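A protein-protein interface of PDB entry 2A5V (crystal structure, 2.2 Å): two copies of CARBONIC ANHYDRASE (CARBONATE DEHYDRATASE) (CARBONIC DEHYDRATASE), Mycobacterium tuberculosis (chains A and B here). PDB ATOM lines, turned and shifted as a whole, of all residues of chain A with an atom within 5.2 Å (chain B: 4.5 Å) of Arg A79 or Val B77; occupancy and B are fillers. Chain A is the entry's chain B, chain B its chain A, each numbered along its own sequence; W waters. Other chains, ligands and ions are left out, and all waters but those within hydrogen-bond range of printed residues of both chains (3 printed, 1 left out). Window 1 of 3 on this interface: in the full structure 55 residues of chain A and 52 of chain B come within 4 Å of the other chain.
Water W2 bridges the side-chain carboxylate of Glu A65 (2.5 Å) and the guanidinium group of Arg B79 (3.0 Å). Water W1 lies within hydrogen-bond range of the guanidinium group of Arg A79 (2.8 Å), the side-chain carboxylate of Glu B65 (2.8 Å), the side-chain carboxylate of Glu A65 (2.9 Å) and the guanidinium group of Arg B79 (2.9 Å). Water W3 bridges the backbone NH of Met B75 (2.9 Å) and the backbone carbonyl oxygen of Ser A60 (2.9 Å).
N of Ala A58 sits at hydrogen-bond distance from O of Thr A80 (2.9 Å). The backbone NH (N) of Val B78 lies within hydrogen-bond range of the backbone carbonyl oxygen (O) of Ile B54 (2.7 Å). The backbone carbonyl oxygen of Ala A58 lies within hydrogen-bond range of the guanidinium group of Arg A79, at 3.3 Å. O of Phe B76 is in hydrogen-bond range of N of Ile B54, 2.8 Å away. The backbone carbonyl oxygen of Cys A57 is in hydrogen-bond range of the guanidinium group of Arg A79. O of Ile A54 sits at hydrogen-bond distance from N of Val A78 (2.8 Å).
Of the 16 printed residues of chain A, 7 touch a printed residue of chain B. Hydrophobic or aromatic side chains of chain A that line the printed part of chain B: Ala A58, Ala A63, Val A77 and Val A78. Along chain A the printed residues that touch a printed residue of chain B span positions 58 to 79. Among the printed residues, 13 pairs touch across the chains. Among the printed residues, Asp or Glu carboxylates within 4 Å of a Lys or Arg side-chain nitrogen of the other chain: Glu A65 with Arg B79 and Arg A79 with Glu B65.
Glu A65 touches Arg B79, and with the chains exchanged Arg A79 touches Glu B65. Val A77 touches Arg B79, and with the chains exchanged Arg A79 touches Val B77. Val A78 touches Arg B79, and with the chains exchanged Arg A79 touches Val B78. Arg B79 touches its own counterpart, Arg A79.
Among the printed residues, merely in contact across the chains: Ala A58 with Phe B76 (3.5 Å), Ser A60 with Met B75 (3.1 Å), Ser A60 with Phe B76 (3.7 Å), Ala A63 with Glu B65 (3.2 Å), Glu A65 with Glu B65 (3.96 Å), Val A77 with Arg B79 (3.2 Å), Val A78 with Arg B79 (3.3 Å), Arg A79 with Val B77 (3.4 Å) and Arg A79 with Val B78 (3.4 Å).
Printed residues of chain B within 4 Å of Glu A65: Glu B65 (3.96 Å) and Arg B79 (2.7 Å). Printed residues of chain B within 4 Å of Val A77: Arg B79. Arg A79 touches just these residues of chain B: Glu B65 (2.8 Å), Val B77 (3.4 Å), Val B78 (3.4 Å) and Arg B79 (3.1 Å). Of the printed residues of chain A, Phe B76 touches Ala A58 and Ser A60. Val B77 touches just these residues of chain A: Ala A58 and Arg A79. Of the printed residues of chain A, Val B78 touches Arg A79 (3.4 Å). The nearest printed residue of chain B that does not touch Arg A79 is Met B75 (4.7 Å). The nearest printed residue of chain A that does not touch Arg B79 is Thr A80 (5.4 Å).
OE2 of Glu B65 lies within salt-bridge range of NH1 of Arg A79, at 2.8 Å. The backbone carbonyl oxygen (O) of Ala A58 lies within hydrogen-bond range of the backbone NH (N) of Val B77 (3.1 Å). O of Arg B79 sits at hydrogen-bond distance from N of Arg A79 (3.1 Å). NH1 of Arg B79 is in salt-bridge range of OE2 of Glu A65 (2.7 Å).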
ATOM      1  N   ILE A  54      -5.772  12.951 -14.949  1.00  0.00           N
ATOM      2  CA  ILE A  54      -5.421  13.157 -16.351  1.00  0.00           C
ATOM      3  C   ILE A  54      -6.672  12.926 -17.163  1.00  0.00           C
ATOM      4  O   ILE A  54      -7.331  11.896 -17.023  1.00  0.00           O
ATOM      5  CB  ILE A  54      -4.265  12.227 -16.846  1.00  0.00           C
ATOM      6  CG1 ILE A  54      -2.874  12.751 -16.453  1.00  0.00           C
ATOM      7  CG2 ILE A  54      -4.252  12.138 -18.412  1.00  0.00           C
ATOM      8  CD1 ILE A  54      -2.709  13.433 -15.082  1.00  0.00           C
ATOM      9  N   PHE A  55      -7.032  13.910 -17.987  1.00  0.00           N
ATOM     10  CA  PHE A  55      -8.078  13.717 -18.969  1.00  0.00           C
ATOM     11  C   PHE A  55      -7.435  13.729 -20.355  1.00  0.00           C
ATOM     12  O   PHE A  55      -7.095  14.795 -20.916  1.00  0.00           O
ATOM     13  CB  PHE A  55      -9.167  14.776 -18.819  1.00  0.00           C
ATOM     14  CG  PHE A  55     -10.301  14.676 -19.859  1.00  0.00           C
ATOM     15  CD1 PHE A  55     -10.802  13.442 -20.277  1.00  0.00           C
ATOM     16  CD2 PHE A  55     -10.879  15.823 -20.370  1.00  0.00           C
ATOM     17  CE1 PHE A  55     -11.828  13.349 -21.221  1.00  0.00           C
ATOM     18  CE2 PHE A  55     -11.933  15.751 -21.315  1.00  0.00           C
ATOM     19  CZ  PHE A  55     -12.432  14.521 -21.711  1.00  0.00           C
ATOM     20  N   GLY A  56      -7.266  12.533 -20.902  1.00  0.00           N
ATOM     21  CA  GLY A  56      -6.456  12.324 -22.098  1.00  0.00           C
ATOM     22  C   GLY A  56      -7.195  11.645 -23.228  1.00  0.00           C
ATOM     23  O   GLY A  56      -8.342  11.222 -23.078  1.00  0.00           O
ATOM     24  N   CYS A  57      -6.539  11.556 -24.384  1.00  0.00           N
ATOM     25  CA  CYS A  57      -7.071  10.752 -25.468  1.00  0.00           C
ATOM     26  C   CYS A  57      -6.914   9.238 -25.191  1.00  0.00           C
ATOM     27  O   CYS A  57      -5.952   8.804 -24.513  1.00  0.00           O
ATOM     28  CB  CYS A  57      -6.405  11.107 -26.762  1.00  0.00           C
ATOM     29  SG  CYS A  57      -7.248  10.382 -28.197  1.00  0.00           S
ATOM     30  N   ALA A  58      -7.869   8.469 -25.707  1.00  0.00           N
ATOM     31  CA  ALA A  58      -7.859   7.013 -25.636  1.00  0.00           C
ATOM     32  C   ALA A  58      -6.751   6.376 -26.486  1.00  0.00           C
ATOM     33  O   ALA A  58      -6.385   5.224 -26.234  1.00  0.00           O
ATOM     34  CB  ALA A  58      -9.237   6.446 -26.044  1.00  0.00           C
ATOM     35  N   ASP A  59      -6.196   7.136 -27.432  1.00  0.00           N
ATOM     36  CA  ASP A  59      -5.085   6.690 -28.289  1.00  0.00           C
ATOM     37  C   ASP A  59      -4.083   5.784 -27.532  1.00  0.00           C
ATOM     38  O   ASP A  59      -3.557   6.174 -26.481  1.00  0.00           O
ATOM     39  CB  ASP A  59      -4.356   7.918 -28.890  1.00  0.00           C
ATOM     40  CG  ASP A  59      -3.372   7.560 -30.005  1.00  0.00           C
ATOM     41  OD1 ASP A  59      -2.427   6.785 -29.798  1.00  0.00           O
ATOM     42  OD2 ASP A  59      -3.526   8.089 -31.125  1.00  0.00           O
ATOM     43  N   SER A  60      -3.826   4.593 -28.070  1.00  0.00           N
ATOM     44  CA  SER A  60      -2.890   3.607 -27.470  1.00  0.00           C
ATOM     45  C   SER A  60      -1.448   4.083 -27.315  1.00  0.00           C
ATOM     46  O   SER A  60      -0.656   3.417 -26.654  1.00  0.00           O
ATOM     47  CB  SER A  60      -2.875   2.303 -28.252  1.00  0.00           C
ATOM     48  OG  SER A  60      -2.302   2.479 -29.525  1.00  0.00           O
ATOM     49  N   VAL A  62      -0.623   7.263 -26.190  1.00  0.00           N
ATOM     50  CA  VAL A  62      -0.607   8.334 -25.209  1.00  0.00           C
ATOM     51  C   VAL A  62      -0.971   7.732 -23.839  1.00  0.00           C
ATOM     52  O   VAL A  62      -1.949   8.144 -23.191  1.00  0.00           O
ATOM     53  CB  VAL A  62      -1.576   9.505 -25.642  1.00  0.00           C
ATOM     54  CG1 VAL A  62      -1.281  10.783 -24.842  1.00  0.00           C
ATOM     55  CG2 VAL A  62      -1.469   9.779 -27.164  1.00  0.00           C
ATOM     56  N   ALA A  63      -0.201   6.726 -23.422  1.00  0.00           N
ATOM     57  CA  ALA A  63      -0.404   6.060 -22.141  1.00  0.00           C
ATOM     58  C   ALA A  63       0.093   6.931 -20.990  1.00  0.00           C
ATOM     59  O   ALA A  63       1.297   6.969 -20.699  1.00  0.00           O
ATOM     60  CB  ALA A  63       0.299   4.701 -22.132  1.00  0.00           C
ATOM     61  N   ALA A  64      -0.861   7.596 -20.343  1.00  0.00           N
ATOM     62  CA  ALA A  64      -0.643   8.708 -19.419  1.00  0.00           C
ATOM     63  C   ALA A  64       0.342   8.396 -18.295  1.00  0.00           C
ATOM     64  O   ALA A  64       1.232   9.194 -18.033  1.00  0.00           O
ATOM     65  CB  ALA A  64      -1.967   9.152 -18.834  1.00  0.00           C
ATOM     66  N   GLU A  65       0.178   7.246 -17.634  1.00  0.00           N
ATOM     67  CA  GLU A  65       1.090   6.857 -16.564  1.00  0.00           C
ATOM     68  C   GLU A  65       2.516   6.653 -17.064  1.00  0.00           C
ATOM     69  O   GLU A  65       3.472   7.005 -16.373  1.00  0.00           O
ATOM     70  CB  GLU A  65       0.604   5.603 -15.828  1.00  0.00           C
ATOM     71  CG  GLU A  65      -0.723   5.786 -15.071  1.00  0.00           C
ATOM     72  CD  GLU A  65      -1.977   5.481 -15.928  1.00  0.00           C
ATOM     73  OE1 GLU A  65      -1.938   5.593 -17.184  1.00  0.00           O
ATOM     74  OE2 GLU A  65      -3.017   5.130 -15.325  1.00  0.00           O
ATOM     75  N   VAL A  77      -7.508   8.643 -13.902  1.00  0.00           N
ATOM     76  CA  VAL A  77      -7.342   8.743 -15.357  1.00  0.00           C
ATOM     77  C   VAL A  77      -8.661   8.594 -16.100  1.00  0.00           C
ATOM     78  O   VAL A  77      -9.360   7.595 -15.975  1.00  0.00           O
ATOM     79  CB  VAL A  77      -6.300   7.730 -15.907  1.00  0.00           C
ATOM     80  CG1 VAL A  77      -6.247   7.756 -17.438  1.00  0.00           C
ATOM     81  CG2 VAL A  77      -4.935   8.010 -15.391  1.00  0.00           C
ATOM     82  N   VAL A  78      -8.980   9.596 -16.894  1.00  0.00           N
ATOM     83  CA  VAL A  78     -10.192   9.609 -17.694  1.00  0.00           C
ATOM     84  C   VAL A  78      -9.752   9.778 -19.116  1.00  0.00           C
ATOM     85  O   VAL A  78      -9.040  10.729 -19.424  1.00  0.00           O
ATOM     86  CB  VAL A  78     -11.155  10.796 -17.268  1.00  0.00           C
ATOM     87  CG1 VAL A  78     -12.475  10.816 -18.103  1.00  0.00           C
ATOM     88  CG2 VAL A  78     -11.448  10.771 -15.753  1.00  0.00           C
ATOM     89  N   ARG A  79     -10.208   8.884 -20.001  1.00  0.00           N
ATOM     90  CA  ARG A  79      -9.730   8.851 -21.385  1.00  0.00           C
ATOM     91  C   ARG A  79     -10.859   8.511 -22.306  1.00  0.00           C
ATOM     92  O   ARG A  79     -11.563   7.531 -22.089  1.00  0.00           O
ATOM     93  CB  ARG A  79      -8.587   7.820 -21.540  1.00  0.00           C
ATOM     94  CG  ARG A  79      -7.266   8.308 -20.951  1.00  0.00           C
ATOM     95  CD  ARG A  79      -6.139   7.267 -20.911  1.00  0.00           C
ATOM     96  NE  ARG A  79      -5.663   6.901 -22.243  1.00  0.00           N
ATOM     97  CZ  ARG A  79      -4.686   6.029 -22.473  1.00  0.00           C
ATOM     98  NH1 ARG A  79      -4.066   5.406 -21.462  1.00  0.00           N
ATOM     99  NH2 ARG A  79      -4.338   5.764 -23.717  1.00  0.00           N
ATOM    100  N   THR A  80     -11.048   9.347 -23.323  1.00  0.00           N
ATOM    101  CA  THR A  80     -12.015   9.119 -24.403  1.00  0.00           C
ATOM    102  C   THR A  80     -11.285   9.509 -25.699  1.00  0.00           C
ATOM    103  O   THR A  80     -10.235  10.130 -25.655  1.00  0.00           O
ATOM    104  CB  THR A  80     -13.303   9.984 -24.262  1.00  0.00           C
ATOM    105  OG1 THR A  80     -12.949  11.366 -24.250  1.00  0.00           O
ATOM    106  CG2 THR A  80     -14.107   9.649 -22.966  1.00  0.00           C
ATOM    107  N   ALA A  81     -11.819   9.128 -26.850  1.00  0.00           N
ATOM    108  CA  ALA A  81     -11.224   9.483 -28.142  1.00  0.00           C
ATOM    109  C   ALA A  81     -11.293  11.015 -28.314  1.00  0.00           C
ATOM    110  O   ALA A  81     -12.373  11.594 -28.204  1.00  0.00           O
ATOM    111  CB  ALA A  81     -11.998   8.785 -29.256  1.00  0.00           C
ATOM    112  N   ILE B  54      -9.027  -1.510 -23.634  1.00  0.00           N
ATOM    113  CA  ILE B  54      -9.424  -1.693 -22.259  1.00  0.00           C
ATOM    114  C   ILE B  54     -10.411  -0.573 -21.914  1.00  0.00           C
ATOM    115  O   ILE B  54     -10.101   0.617 -22.092  1.00  0.00           O
ATOM    116  CB  ILE B  54      -8.238  -1.734 -21.264  1.00  0.00           C
ATOM    117  CG1 ILE B  54      -7.477  -3.070 -21.287  1.00  0.00           C
ATOM    118  CG2 ILE B  54      -8.740  -1.644 -19.851  1.00  0.00           C
ATOM    119  CD1 ILE B  54      -7.205  -3.685 -22.624  1.00  0.00           C
ATOM    120  N   GLU B  65      -2.275  -0.257 -18.490  1.00  0.00           N
ATOM    121  CA  GLU B  65      -0.996  -0.642 -19.102  1.00  0.00           C
ATOM    122  C   GLU B  65      -0.010  -1.247 -18.108  1.00  0.00           C
ATOM    123  O   GLU B  65       0.737  -2.194 -18.432  1.00  0.00           O
ATOM    124  CB  GLU B  65      -0.345   0.536 -19.845  1.00  0.00           C
ATOM    125  CG  GLU B  65      -1.198   1.107 -21.003  1.00  0.00           C
ATOM    126  CD  GLU B  65      -2.099   2.286 -20.574  1.00  0.00           C
ATOM    127  OE1 GLU B  65      -2.530   2.375 -19.410  1.00  0.00           O
ATOM    128  OE2 GLU B  65      -2.365   3.153 -21.405  1.00  0.00           O
ATOM    129  N   MET B  75      -2.611  -0.955 -26.257  1.00  0.00           N
ATOM    130  CA  MET B  75      -4.024  -0.918 -25.915  1.00  0.00           C
ATOM    131  C   MET B  75      -4.613   0.481 -26.012  1.00  0.00           C
ATOM    132  O   MET B  75      -4.028   1.457 -25.512  1.00  0.00           O
ATOM    133  CB  MET B  75      -4.262  -1.540 -24.533  1.00  0.00           C
ATOM    134  CG  MET B  75      -3.463  -0.878 -23.406  1.00  0.00           C
ATOM    135  SD  MET B  75      -4.036  -1.340 -21.760  1.00  0.00           S
ATOM    136  CE  MET B  75      -3.568  -3.067 -21.734  1.00  0.00           C
ATOM    137  N   PHE B  76      -5.734   0.556 -26.715  1.00  0.00           N
ATOM    138  CA  PHE B  76      -6.621   1.698 -26.720  1.00  0.00           C
ATOM    139  C   PHE B  76      -7.334   1.664 -25.356  1.00  0.00           C
ATOM    140  O   PHE B  76      -7.766   0.612 -24.908  1.00  0.00           O
ATOM    141  CB  PHE B  76      -7.592   1.485 -27.872  1.00  0.00           C
ATOM    142  CG  PHE B  76      -8.405   2.685 -28.255  1.00  0.00           C
ATOM    143  CD1 PHE B  76      -7.926   3.617 -29.165  1.00  0.00           C
ATOM    144  CD2 PHE B  76      -9.700   2.860 -27.740  1.00  0.00           C
ATOM    145  CE1 PHE B  76      -8.733   4.701 -29.556  1.00  0.00           C
ATOM    146  CE2 PHE B  76     -10.512   3.930 -28.149  1.00  0.00           C
ATOM    147  CZ  PHE B  76     -10.029   4.850 -29.037  1.00  0.00           C
ATOM    148  N   VAL B  77      -7.364   2.789 -24.644  1.00  0.00           N
ATOM    149  CA  VAL B  77      -7.846   2.786 -23.261  1.00  0.00           C
ATOM    150  C   VAL B  77      -8.972   3.782 -23.091  1.00  0.00           C
ATOM    151  O   VAL B  77      -8.816   4.938 -23.380  1.00  0.00           O
ATOM    152  CB  VAL B  77      -6.691   3.054 -22.255  1.00  0.00           C
ATOM    153  CG1 VAL B  77      -7.209   3.183 -20.806  1.00  0.00           C
ATOM    154  CG2 VAL B  77      -5.670   1.904 -22.338  1.00  0.00           C
ATOM    155  N   VAL B  78     -10.127   3.298 -22.646  1.00  0.00           N
ATOM    156  CA  VAL B  78     -11.250   4.146 -22.300  1.00  0.00           C
ATOM    157  C   VAL B  78     -11.478   3.998 -20.796  1.00  0.00           C
ATOM    158  O   VAL B  78     -11.618   2.888 -20.280  1.00  0.00           O
ATOM    159  CB  VAL B  78     -12.503   3.823 -23.188  1.00  0.00           C
ATOM    160  CG1 VAL B  78     -13.720   4.744 -22.854  1.00  0.00           C
ATOM    161  CG2 VAL B  78     -12.121   3.968 -24.632  1.00  0.00           C
ATOM    162  N   ARG B  79     -11.449   5.103 -20.070  1.00  0.00           N
ATOM    163  CA  ARG B  79     -11.580   5.016 -18.618  1.00  0.00           C
ATOM    164  C   ARG B  79     -12.543   6.094 -18.130  1.00  0.00           C
ATOM    165  O   ARG B  79     -12.378   7.273 -18.487  1.00  0.00           O
ATOM    166  CB  ARG B  79     -10.211   5.173 -17.948  1.00  0.00           C
ATOM    167  CG  ARG B  79      -9.400   3.893 -17.897  1.00  0.00           C
ATOM    168  CD  ARG B  79      -7.938   4.114 -17.530  1.00  0.00           C
ATOM    169  NE  ARG B  79      -7.785   4.208 -16.090  1.00  0.00           N
ATOM    170  CZ  ARG B  79      -6.636   4.368 -15.456  1.00  0.00           C
ATOM    171  NH1 ARG B  79      -5.488   4.423 -16.131  1.00  0.00           N
ATOM    172  NH2 ARG B  79      -6.639   4.458 -14.131  1.00  0.00           N
HETATM  173  O   HOH W   1      -4.178   4.582 -18.765  1.00  0.00           O
HETATM  174  O   HOH W   2      -4.008   5.304 -13.030  1.00  0.00           O
HETATM  175  O   HOH W   3      -0.884   0.994 -25.073  1.00  0.00           O
